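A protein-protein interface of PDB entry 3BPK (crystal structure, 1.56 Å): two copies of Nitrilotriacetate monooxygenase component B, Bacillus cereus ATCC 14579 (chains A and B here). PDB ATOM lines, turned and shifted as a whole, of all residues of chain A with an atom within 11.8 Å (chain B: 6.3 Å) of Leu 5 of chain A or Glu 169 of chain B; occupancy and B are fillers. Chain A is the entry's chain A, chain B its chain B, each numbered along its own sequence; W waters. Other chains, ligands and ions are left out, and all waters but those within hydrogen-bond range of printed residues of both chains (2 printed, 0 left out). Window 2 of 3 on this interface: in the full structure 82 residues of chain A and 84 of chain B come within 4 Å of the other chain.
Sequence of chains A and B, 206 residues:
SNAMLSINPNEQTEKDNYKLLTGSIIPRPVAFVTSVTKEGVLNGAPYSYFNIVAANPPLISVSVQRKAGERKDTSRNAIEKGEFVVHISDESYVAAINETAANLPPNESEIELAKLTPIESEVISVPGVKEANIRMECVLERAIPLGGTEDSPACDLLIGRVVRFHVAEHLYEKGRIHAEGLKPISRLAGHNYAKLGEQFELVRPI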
ATOM      1  N   ALA A   3      18.640 -13.724  12.006  1.00  0.00           N
ATOM      2  CA  ALA A   3      17.444 -14.396  12.620  1.00  0.00           C
ATOM      3  C   ALA A   3      17.675 -14.761  14.088  1.00  0.00           C
ATOM      4  O   ALA A   3      16.735 -15.273  14.705  1.00  0.00           O
ATOM      5  CB  ALA A   3      17.052 -15.654  11.849  1.00  0.00           C
ATOM      6  N   MET A   4      18.907 -14.529  14.598  1.00  0.00           N
ATOM      7  CA  MET A   4      19.250 -14.671  16.031  1.00  0.00           C
ATOM      8  C   MET A   4      19.701 -13.337  16.605  1.00  0.00           C
ATOM      9  O   MET A   4      20.547 -12.621  15.983  1.00  0.00           O
ATOM     10  CB  MET A   4      20.384 -15.694  16.250  1.00  0.00           C
ATOM     11  CG  MET A   4      20.103 -17.107  15.748  1.00  0.00           C
ATOM     12  SD  MET A   4      18.754 -18.081  16.830  1.00  0.00           S
ATOM     13  CE  MET A   4      19.767 -18.318  18.492  1.00  0.00           C
ATOM     14  N   LEU A   5      19.184 -13.002  17.786  1.00  0.00           N
ATOM     15  CA  LEU A   5      19.578 -11.818  18.541  1.00  0.00           C
ATOM     16  C   LEU A   5      20.704 -12.175  19.498  1.00  0.00           C
ATOM     17  O   LEU A   5      20.632 -13.212  20.180  1.00  0.00           O
ATOM     18  CB  LEU A   5      18.393 -11.264  19.357  1.00  0.00           C
ATOM     19  CG  LEU A   5      17.099 -10.986  18.586  1.00  0.00           C
ATOM     20  CD1 LEU A   5      15.972 -10.531  19.513  1.00  0.00           C
ATOM     21  CD2 LEU A   5      17.343  -9.963  17.465  1.00  0.00           C
ATOM     22  N   SER A   6      21.693 -11.297  19.601  1.00  0.00           N
ATOM     23  CA  SER A   6      22.803 -11.446  20.559  1.00  0.00           C
ATOM     24  C   SER A   6      22.688 -10.402  21.672  1.00  0.00           C
ATOM     25  O   SER A   6      22.717  -9.203  21.417  1.00  0.00           O
ATOM     26  CB  SER A   6      24.159 -11.327  19.856  1.00  0.00           C
ATOM     27  OG  SER A   6      25.209 -11.275  20.798  1.00  0.00           O
ATOM     28  N   ILE A   7      22.533 -10.870  22.908  1.00  0.00           N
ATOM     29  CA  ILE A   7      22.248  -9.999  24.037  1.00  0.00           C
ATOM     30  C   ILE A   7      23.257 -10.195  25.148  1.00  0.00           C
ATOM     31  O   ILE A   7      23.400 -11.300  25.708  1.00  0.00           O
ATOM     32  CB  ILE A   7      20.788 -10.262  24.540  1.00  0.00           C
ATOM     33  CG1 ILE A   7      19.768  -9.932  23.433  1.00  0.00           C
ATOM     34  CG2 ILE A   7      20.500  -9.495  25.836  1.00  0.00           C
ATOM     35  CD1 ILE A   7      18.361 -10.454  23.696  1.00  0.00           C
ATOM     36  N   ASN A   8      23.965  -9.129  25.463  1.00  0.00           N
ATOM     37  CA  ASN A   8      24.937  -9.116  26.555  1.00  0.00           C
ATOM     38  C   ASN A   8      24.233  -8.847  27.887  1.00  0.00           C
ATOM     39  O   ASN A   8      23.686  -7.763  28.112  1.00  0.00           O
ATOM     40  CB  ASN A   8      25.982  -8.017  26.282  1.00  0.00           C
ATOM     41  CG  ASN A   8      27.068  -7.977  27.332  1.00  0.00           C
ATOM     42  OD1 ASN A   8      27.004  -8.706  28.331  1.00  0.00           O
ATOM     43  ND2 ASN A   8      28.078  -7.116  27.125  1.00  0.00           N
ATOM     44  N   PRO A   9      24.280  -9.827  28.804  1.00  0.00           N
ATOM     45  CA  PRO A   9      23.560  -9.608  30.056  1.00  0.00           C
ATOM     46  C   PRO A   9      24.127  -8.433  30.871  1.00  0.00           C
ATOM     47  O   PRO A   9      23.383  -7.863  31.677  1.00  0.00           O
ATOM     48  CB  PRO A   9      23.746 -10.952  30.826  1.00  0.00           C
ATOM     49  CG  PRO A   9      25.000 -11.545  30.241  1.00  0.00           C
ATOM     50  CD  PRO A   9      24.958 -11.154  28.758  1.00  0.00           C
ATOM     51  N   GLN A  12      22.222  -5.098  29.995  1.00  0.00           N
ATOM     52  CA  GLN A  12      20.836  -4.932  30.351  1.00  0.00           C
ATOM     53  C   GLN A  12      20.641  -5.017  31.860  1.00  0.00           C
ATOM     54  O   GLN A  12      21.620  -5.184  32.614  1.00  0.00           O
ATOM     55  CB  GLN A  12      19.933  -5.867  29.519  1.00  0.00           C
ATOM     56  CG  GLN A  12      20.144  -7.328  29.699  1.00  0.00           C
ATOM     57  CD  GLN A  12      19.154  -8.136  28.864  1.00  0.00           C
ATOM     58  OE1 GLN A  12      18.495  -7.616  27.951  1.00  0.00           O
ATOM     59  NE2 GLN A  12      19.005  -9.401  29.212  1.00  0.00           N
ATOM     60  N   ASP A  16      15.703  -7.368  33.144  1.00  0.00           N
ATOM     61  CA  ASP A  16      15.791  -7.850  31.760  1.00  0.00           C
ATOM     62  C   ASP A  16      16.337  -9.296  31.756  1.00  0.00           C
ATOM     63  O   ASP A  16      15.845 -10.160  31.004  1.00  0.00           O
ATOM     64  CB  ASP A  16      16.723  -6.980  30.910  1.00  0.00           C
ATOM     65  CG  ASP A  16      16.194  -5.557  30.705  1.00  0.00           C
ATOM     66  OD1 ASP A  16      14.960  -5.379  30.616  1.00  0.00           O
ATOM     67  OD2 ASP A  16      17.047  -4.620  30.629  1.00  0.00           O
ATOM     68  N   ASN A  17      17.359  -9.539  32.586  1.00  0.00           N
ATOM     69  CA  ASN A  17      17.958 -10.875  32.622  1.00  0.00           C
ATOM     70  C   ASN A  17      17.003 -11.876  33.244  1.00  0.00           C
ATOM     71  O   ASN A  17      16.884 -13.030  32.776  1.00  0.00           O
ATOM     72  CB  ASN A  17      19.288 -10.847  33.377  1.00  0.00           C
ATOM     73  CG  ASN A  17      20.376 -10.134  32.588  1.00  0.00           C
ATOM     74  OD1 ASN A  17      20.500 -10.328  31.364  1.00  0.00           O
ATOM     75  ND2 ASN A  17      21.199  -9.330  33.281  1.00  0.00           N
ATOM     76  N   LEU A  20      14.510 -12.971  30.649  1.00  0.00           N
ATOM     77  CA  LEU A  20      15.018 -13.944  29.650  1.00  0.00           C
ATOM     78  C   LEU A  20      15.215 -15.321  30.295  1.00  0.00           C
ATOM     79  O   LEU A  20      14.906 -16.358  29.679  1.00  0.00           O
ATOM     80  CB  LEU A  20      16.354 -13.519  29.088  1.00  0.00           C
ATOM     81  CG  LEU A  20      16.334 -12.477  28.025  1.00  0.00           C
ATOM     82  CD1 LEU A  20      17.714 -12.382  27.417  1.00  0.00           C
ATOM     83  CD2 LEU A  20      15.285 -12.855  26.969  1.00  0.00           C
ATOM     84  N   SER A  24      12.952 -18.568  29.152  1.00  0.00           N
ATOM     85  CA  SER A  24      13.710 -19.561  28.360  1.00  0.00           C
ATOM     86  C   SER A  24      13.806 -20.923  29.022  1.00  0.00           C
ATOM     87  O   SER A  24      13.651 -21.964  28.352  1.00  0.00           O
ATOM     88  CB  SER A  24      15.134 -19.056  28.069  1.00  0.00           C
ATOM     89  OG  SER A  24      15.154 -17.804  27.384  1.00  0.00           O
ATOM     90  N   ASN B 133      17.123 -22.667  19.271  1.00  0.00           N
ATOM     91  CA  ASN B 133      16.489 -21.363  19.160  1.00  0.00           C
ATOM     92  C   ASN B 133      16.905 -20.417  20.310  1.00  0.00           C
ATOM     93  O   ASN B 133      16.779 -19.202  20.209  1.00  0.00           O
ATOM     94  CB  ASN B 133      14.965 -21.545  19.072  1.00  0.00           C
ATOM     95  CG  ASN B 133      14.540 -22.224  17.761  1.00  0.00           C
ATOM     96  OD1 ASN B 133      14.410 -21.549  16.740  1.00  0.00           O
ATOM     97  ND2 ASN B 133      14.334 -23.551  17.781  1.00  0.00           N
ATOM     98  N   PHE B 165      23.480 -14.239  25.778  1.00  0.00           N
ATOM     99  CA  PHE B 165      22.249 -14.903  25.375  1.00  0.00           C
ATOM    100  C   PHE B 165      22.158 -14.787  23.858  1.00  0.00           C
ATOM    101  O   PHE B 165      22.482 -13.716  23.301  1.00  0.00           O
ATOM    102  CB  PHE B 165      21.028 -14.184  25.906  1.00  0.00           C
ATOM    103  CG  PHE B 165      20.782 -14.355  27.378  1.00  0.00           C
ATOM    104  CD1 PHE B 165      20.126 -15.486  27.858  1.00  0.00           C
ATOM    105  CD2 PHE B 165      21.116 -13.335  28.275  1.00  0.00           C
ATOM    106  CE1 PHE B 165      19.812 -15.603  29.228  1.00  0.00           C
ATOM    107  CE2 PHE B 165      20.831 -13.461  29.626  1.00  0.00           C
ATOM    108  CZ  PHE B 165      20.172 -14.606  30.099  1.00  0.00           C
ATOM    109  N   HIS B 166      21.696 -15.857  23.197  1.00  0.00           N
ATOM    110  CA  HIS B 166      21.385 -15.856  21.759  1.00  0.00           C
ATOM    111  C   HIS B 166      19.949 -16.330  21.649  1.00  0.00           C
ATOM    112  O   HIS B 166      19.627 -17.424  22.107  1.00  0.00           O
ATOM    113  CB  HIS B 166      22.268 -16.836  21.015  1.00  0.00           C
ATOM    114  CG  HIS B 166      23.730 -16.508  21.098  1.00  0.00           C
ATOM    115  ND1 HIS B 166      24.329 -15.598  20.253  1.00  0.00           N
ATOM    116  CD2 HIS B 166      24.693 -16.920  21.960  1.00  0.00           C
ATOM    117  CE1 HIS B 166      25.615 -15.493  20.571  1.00  0.00           C
ATOM    118  NE2 HIS B 166      25.858 -16.279  21.611  1.00  0.00           N
ATOM    119  N   VAL B 167      19.070 -15.502  21.077  1.00  0.00           N
ATOM    120  CA  VAL B 167      17.629 -15.787  21.076  1.00  0.00           C
ATOM    121  C   VAL B 167      17.038 -15.593  19.692  1.00  0.00           C
ATOM    122  O   VAL B 167      17.260 -14.541  19.093  1.00  0.00           O
ATOM    123  CB  VAL B 167      16.867 -14.870  22.068  1.00  0.00           C
ATOM    124  CG1 VAL B 167      15.363 -15.182  22.054  1.00  0.00           C
ATOM    125  CG2 VAL B 167      17.468 -14.955  23.526  1.00  0.00           C
ATOM    126  N   ALA B 168      16.294 -16.572  19.185  1.00  0.00           N
ATOM    127  CA  ALA B 168      15.655 -16.414  17.866  1.00  0.00           C
ATOM    128  C   ALA B 168      14.725 -15.195  17.872  1.00  0.00           C
ATOM    129  O   ALA B 168      13.897 -15.030  18.770  1.00  0.00           O
ATOM    130  CB  ALA B 168      14.900 -17.694  17.467  1.00  0.00           C
ATOM    131  N   GLU B 169      14.872 -14.327  16.850  1.00  0.00           N
ATOM    132  CA  GLU B 169      14.130 -13.076  16.863  1.00  0.00           C
ATOM    133  C   GLU B 169      12.626 -13.354  16.887  1.00  0.00           C
ATOM    134  O   GLU B 169      11.878 -12.617  17.556  1.00  0.00           O
ATOM    135  CB  GLU B 169      14.505 -12.178  15.669  1.00  0.00           C
ATOM    136  CG  GLU B 169      13.879 -10.763  15.732  1.00  0.00           C
ATOM    137  CD  GLU B 169      12.462 -10.654  15.122  1.00  0.00           C
ATOM    138  OE1 GLU B 169      11.971 -11.616  14.485  1.00  0.00           O
ATOM    139  OE2 GLU B 169      11.842  -9.578  15.287  1.00  0.00           O
ATOM    140  N   HIS B 170      12.183 -14.411  16.202  1.00  0.00           N
ATOM    141  CA  HIS B 170      10.741 -14.703  16.178  1.00  0.00           C
ATOM    142  C   HIS B 170      10.134 -15.085  17.526  1.00  0.00           C
ATOM    143  O   HIS B 170       8.901 -15.059  17.664  1.00  0.00           O
ATOM    144  CB  HIS B 170      10.360 -15.751  15.118  1.00  0.00           C
ATOM    145  CG  HIS B 170      10.782 -17.145  15.474  1.00  0.00           C
ATOM    146  ND1 HIS B 170      12.047 -17.631  15.205  1.00  0.00           N
ATOM    147  CD2 HIS B 170      10.116 -18.153  16.088  1.00  0.00           C
ATOM    148  CE1 HIS B 170      12.139 -18.878  15.638  1.00  0.00           C
ATOM    149  NE2 HIS B 170      10.982 -19.219  16.175  1.00  0.00           N
ATOM    150  N   LEU B 171      10.989 -15.450  18.491  1.00  0.00           N
ATOM    151  CA  LEU B 171      10.542 -15.820  19.845  1.00  0.00           C
ATOM    152  C   LEU B 171      10.530 -14.658  20.822  1.00  0.00           C
ATOM    153  O   LEU B 171       9.981 -14.752  21.915  1.00  0.00           O
ATOM    154  CB  LEU B 171      11.477 -16.919  20.438  1.00  0.00           C
ATOM    155  CG  LEU B 171      11.439 -18.242  19.685  1.00  0.00           C
ATOM    156  CD1 LEU B 171      12.411 -19.236  20.322  1.00  0.00           C
ATOM    157  CD2 LEU B 171      10.017 -18.799  19.657  1.00  0.00           C
ATOM    158  N   TYR B 172      11.174 -13.563  20.456  1.00  0.00           N
ATOM    159  CA  TYR B 172      11.457 -12.515  21.422  1.00  0.00           C
ATOM    160  C   TYR B 172      10.477 -11.372  21.227  1.00  0.00           C
ATOM    161  O   TYR B 172      10.275 -10.929  20.085  1.00  0.00           O
ATOM    162  CB  TYR B 172      12.885 -12.038  21.190  1.00  0.00           C
ATOM    163  CG  TYR B 172      13.380 -10.992  22.150  1.00  0.00           C
ATOM    164  CD1 TYR B 172      14.210 -11.330  23.226  1.00  0.00           C
ATOM    165  CD2 TYR B 172      13.031  -9.653  21.982  1.00  0.00           C
ATOM    166  CE1 TYR B 172      14.680 -10.373  24.085  1.00  0.00           C
ATOM    167  CE2 TYR B 172      13.501  -8.680  22.845  1.00  0.00           C
ATOM    168  CZ  TYR B 172      14.345  -9.042  23.892  1.00  0.00           C
ATOM    169  OH  TYR B 172      14.810  -8.075  24.755  1.00  0.00           O
ATOM    170  N   GLU B 173       9.842 -10.941  22.314  1.00  0.00           N
ATOM    171  CA  GLU B 173       8.880  -9.831  22.254  1.00  0.00           C
ATOM    172  C   GLU B 173       8.932  -9.025  23.543  1.00  0.00           C
ATOM    173  O   GLU B 173       8.548  -9.529  24.605  1.00  0.00           O
ATOM    174  CB  GLU B 173       7.461 -10.372  22.000  1.00  0.00           C
ATOM    175  CG  GLU B 173       6.301  -9.376  22.259  1.00  0.00           C
ATOM    176  CD  GLU B 173       6.209  -8.276  21.228  1.00  0.00           C
ATOM    177  OE1 GLU B 173       5.070  -7.982  20.781  1.00  0.00           O
ATOM    178  OE2 GLU B 173       7.258  -7.697  20.870  1.00  0.00           O
HETATM  179  O   HOH W   1      16.394  -9.013  26.746  1.00  0.00           O
HETATM  180  O   HOH W   2      13.837 -15.908  14.112  1.00  0.00           O
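Of the printed residues of chain B, Leu 5 of chain A touches Phe 165, His 166, Val 167, Glu 169 and Tyr 172.
Of the printed residues of chain B, Ser 6 of chain A touches Phe 165 (3.6 Å).
Gln 12 of chain A touches none of the printed residues of chain B.
Of the printed residues of chain B, Leu 20 of chain A touches Phe 165 (3.6 Å) and Tyr 172 (3.9 Å).
Of the printed residues of chain A, Phe 165 of chain B touches Leu 5, Ser 6, Ile 7, Asn 17 and Leu 20.
Printed residues of chain A within 4 Å of His 166 of chain B: Met 4 (3.7 Å) and Leu 5 (3.2 Å).
Of chain A, only Met 4 and Leu 5 come within 4 Å of Val 167 of chain B.
Of the printed residues of chain A, Glu 169 of chain B touches Ala 3 and Leu 5.
No residue of chain A comes within 4 Å of His 170 of chain B.
The nearest printed residue of chain B that does not touch Leu 5 of chain A is Ala 168 of chain B (4.8 Å).
Ala 168 of chain B touches Ala 3 of chain A.
Met 4 of chain A touches Asn 133 of chain B (CE to O, 3.6 Å).
His 166 of chain B touches Met 4 of chain A.
Met 4 of chain A touches Val 167 of chain B (CA to O, 3.7 Å).
Leu 5 of chain A touches His 166 of chain B (O to CA, 3.2 Å).
Glu 169 of chain B touches Leu 5 of chain A (CG to CD2, 3.96 Å).
O of Phe 165 of chain B touches CA of Ser 6 of chain A (3.6 Å).
Ile 7 of chain A touches Tyr 172 of chain B (CD1 to CE1, 3.7 Å).
OD1 of Asn 17 of chain A touches CE2 of Phe 165 of chain B (3.6 Å).
Leu 20 of chain A touches Tyr 172 of chain B (CD2 to CE1, 3.9 Å).
Water W1 bridges the side-chain hydroxyl of Tyr 172 of chain B and the side-chain amide oxygen of Gln 12 of chain A.
Water W2 lies within hydrogen-bond range of ND1 of His 170 of chain B, O of Ala 3 of chain A and N of Glu 169 of chain B.
The backbone carbonyl oxygen (O) of Ala 3 of chain A is in hydrogen-bond range of the backbone NH (N) of Glu 169 of chain B (3.0 Å).
The side-chain sulfur (SD) of Met 4 of chain A lies close to the backbone NH (N) of Ala 168 of chain B, at 3.7 Å.
N of Leu 5 of chain A is in hydrogen-bond range of O of Val 167 of chain B, at 2.8 Å.
The backbone NH (N) of Ile 7 of chain A lies within hydrogen-bond range of the backbone carbonyl oxygen (O) of Phe 165 of chain B (2.9 Å).
O of Pro 9 of chain A is in hydrogen-bond range of ND2 of Asn 17 of chain A.
OD1 of Asn 17 of chain A is in hydrogen-bond range of NE2 of Gln 12 of chain A, 2.8 Å away.
The backbone carbonyl oxygen (O) of Leu 20 of chain A sits at hydrogen-bond distance from the side-chain hydroxyl (OG) of Ser 24 of chain A, at 2.7 Å.
The backbone carbonyl oxygen (O) of Asn 133 of chain B lies within hydrogen-bond range of the backbone NH (N) of Ala 168 of chain B, 2.9 Å away.
No position is printed for both chains.
Of the 17 pairs that touch across the chains among the printed residues, none has its exchanged pair printed and touching as well.
Of the 10 printed residues of chain B, 7 touch a printed residue of chain A.
Among the printed residues, 17 pairs touch across the chains.
Among the printed residues, no Asp or Glu carboxylate lies within 4 Å of a Lys or Arg side-chain nitrogen of the other chain.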
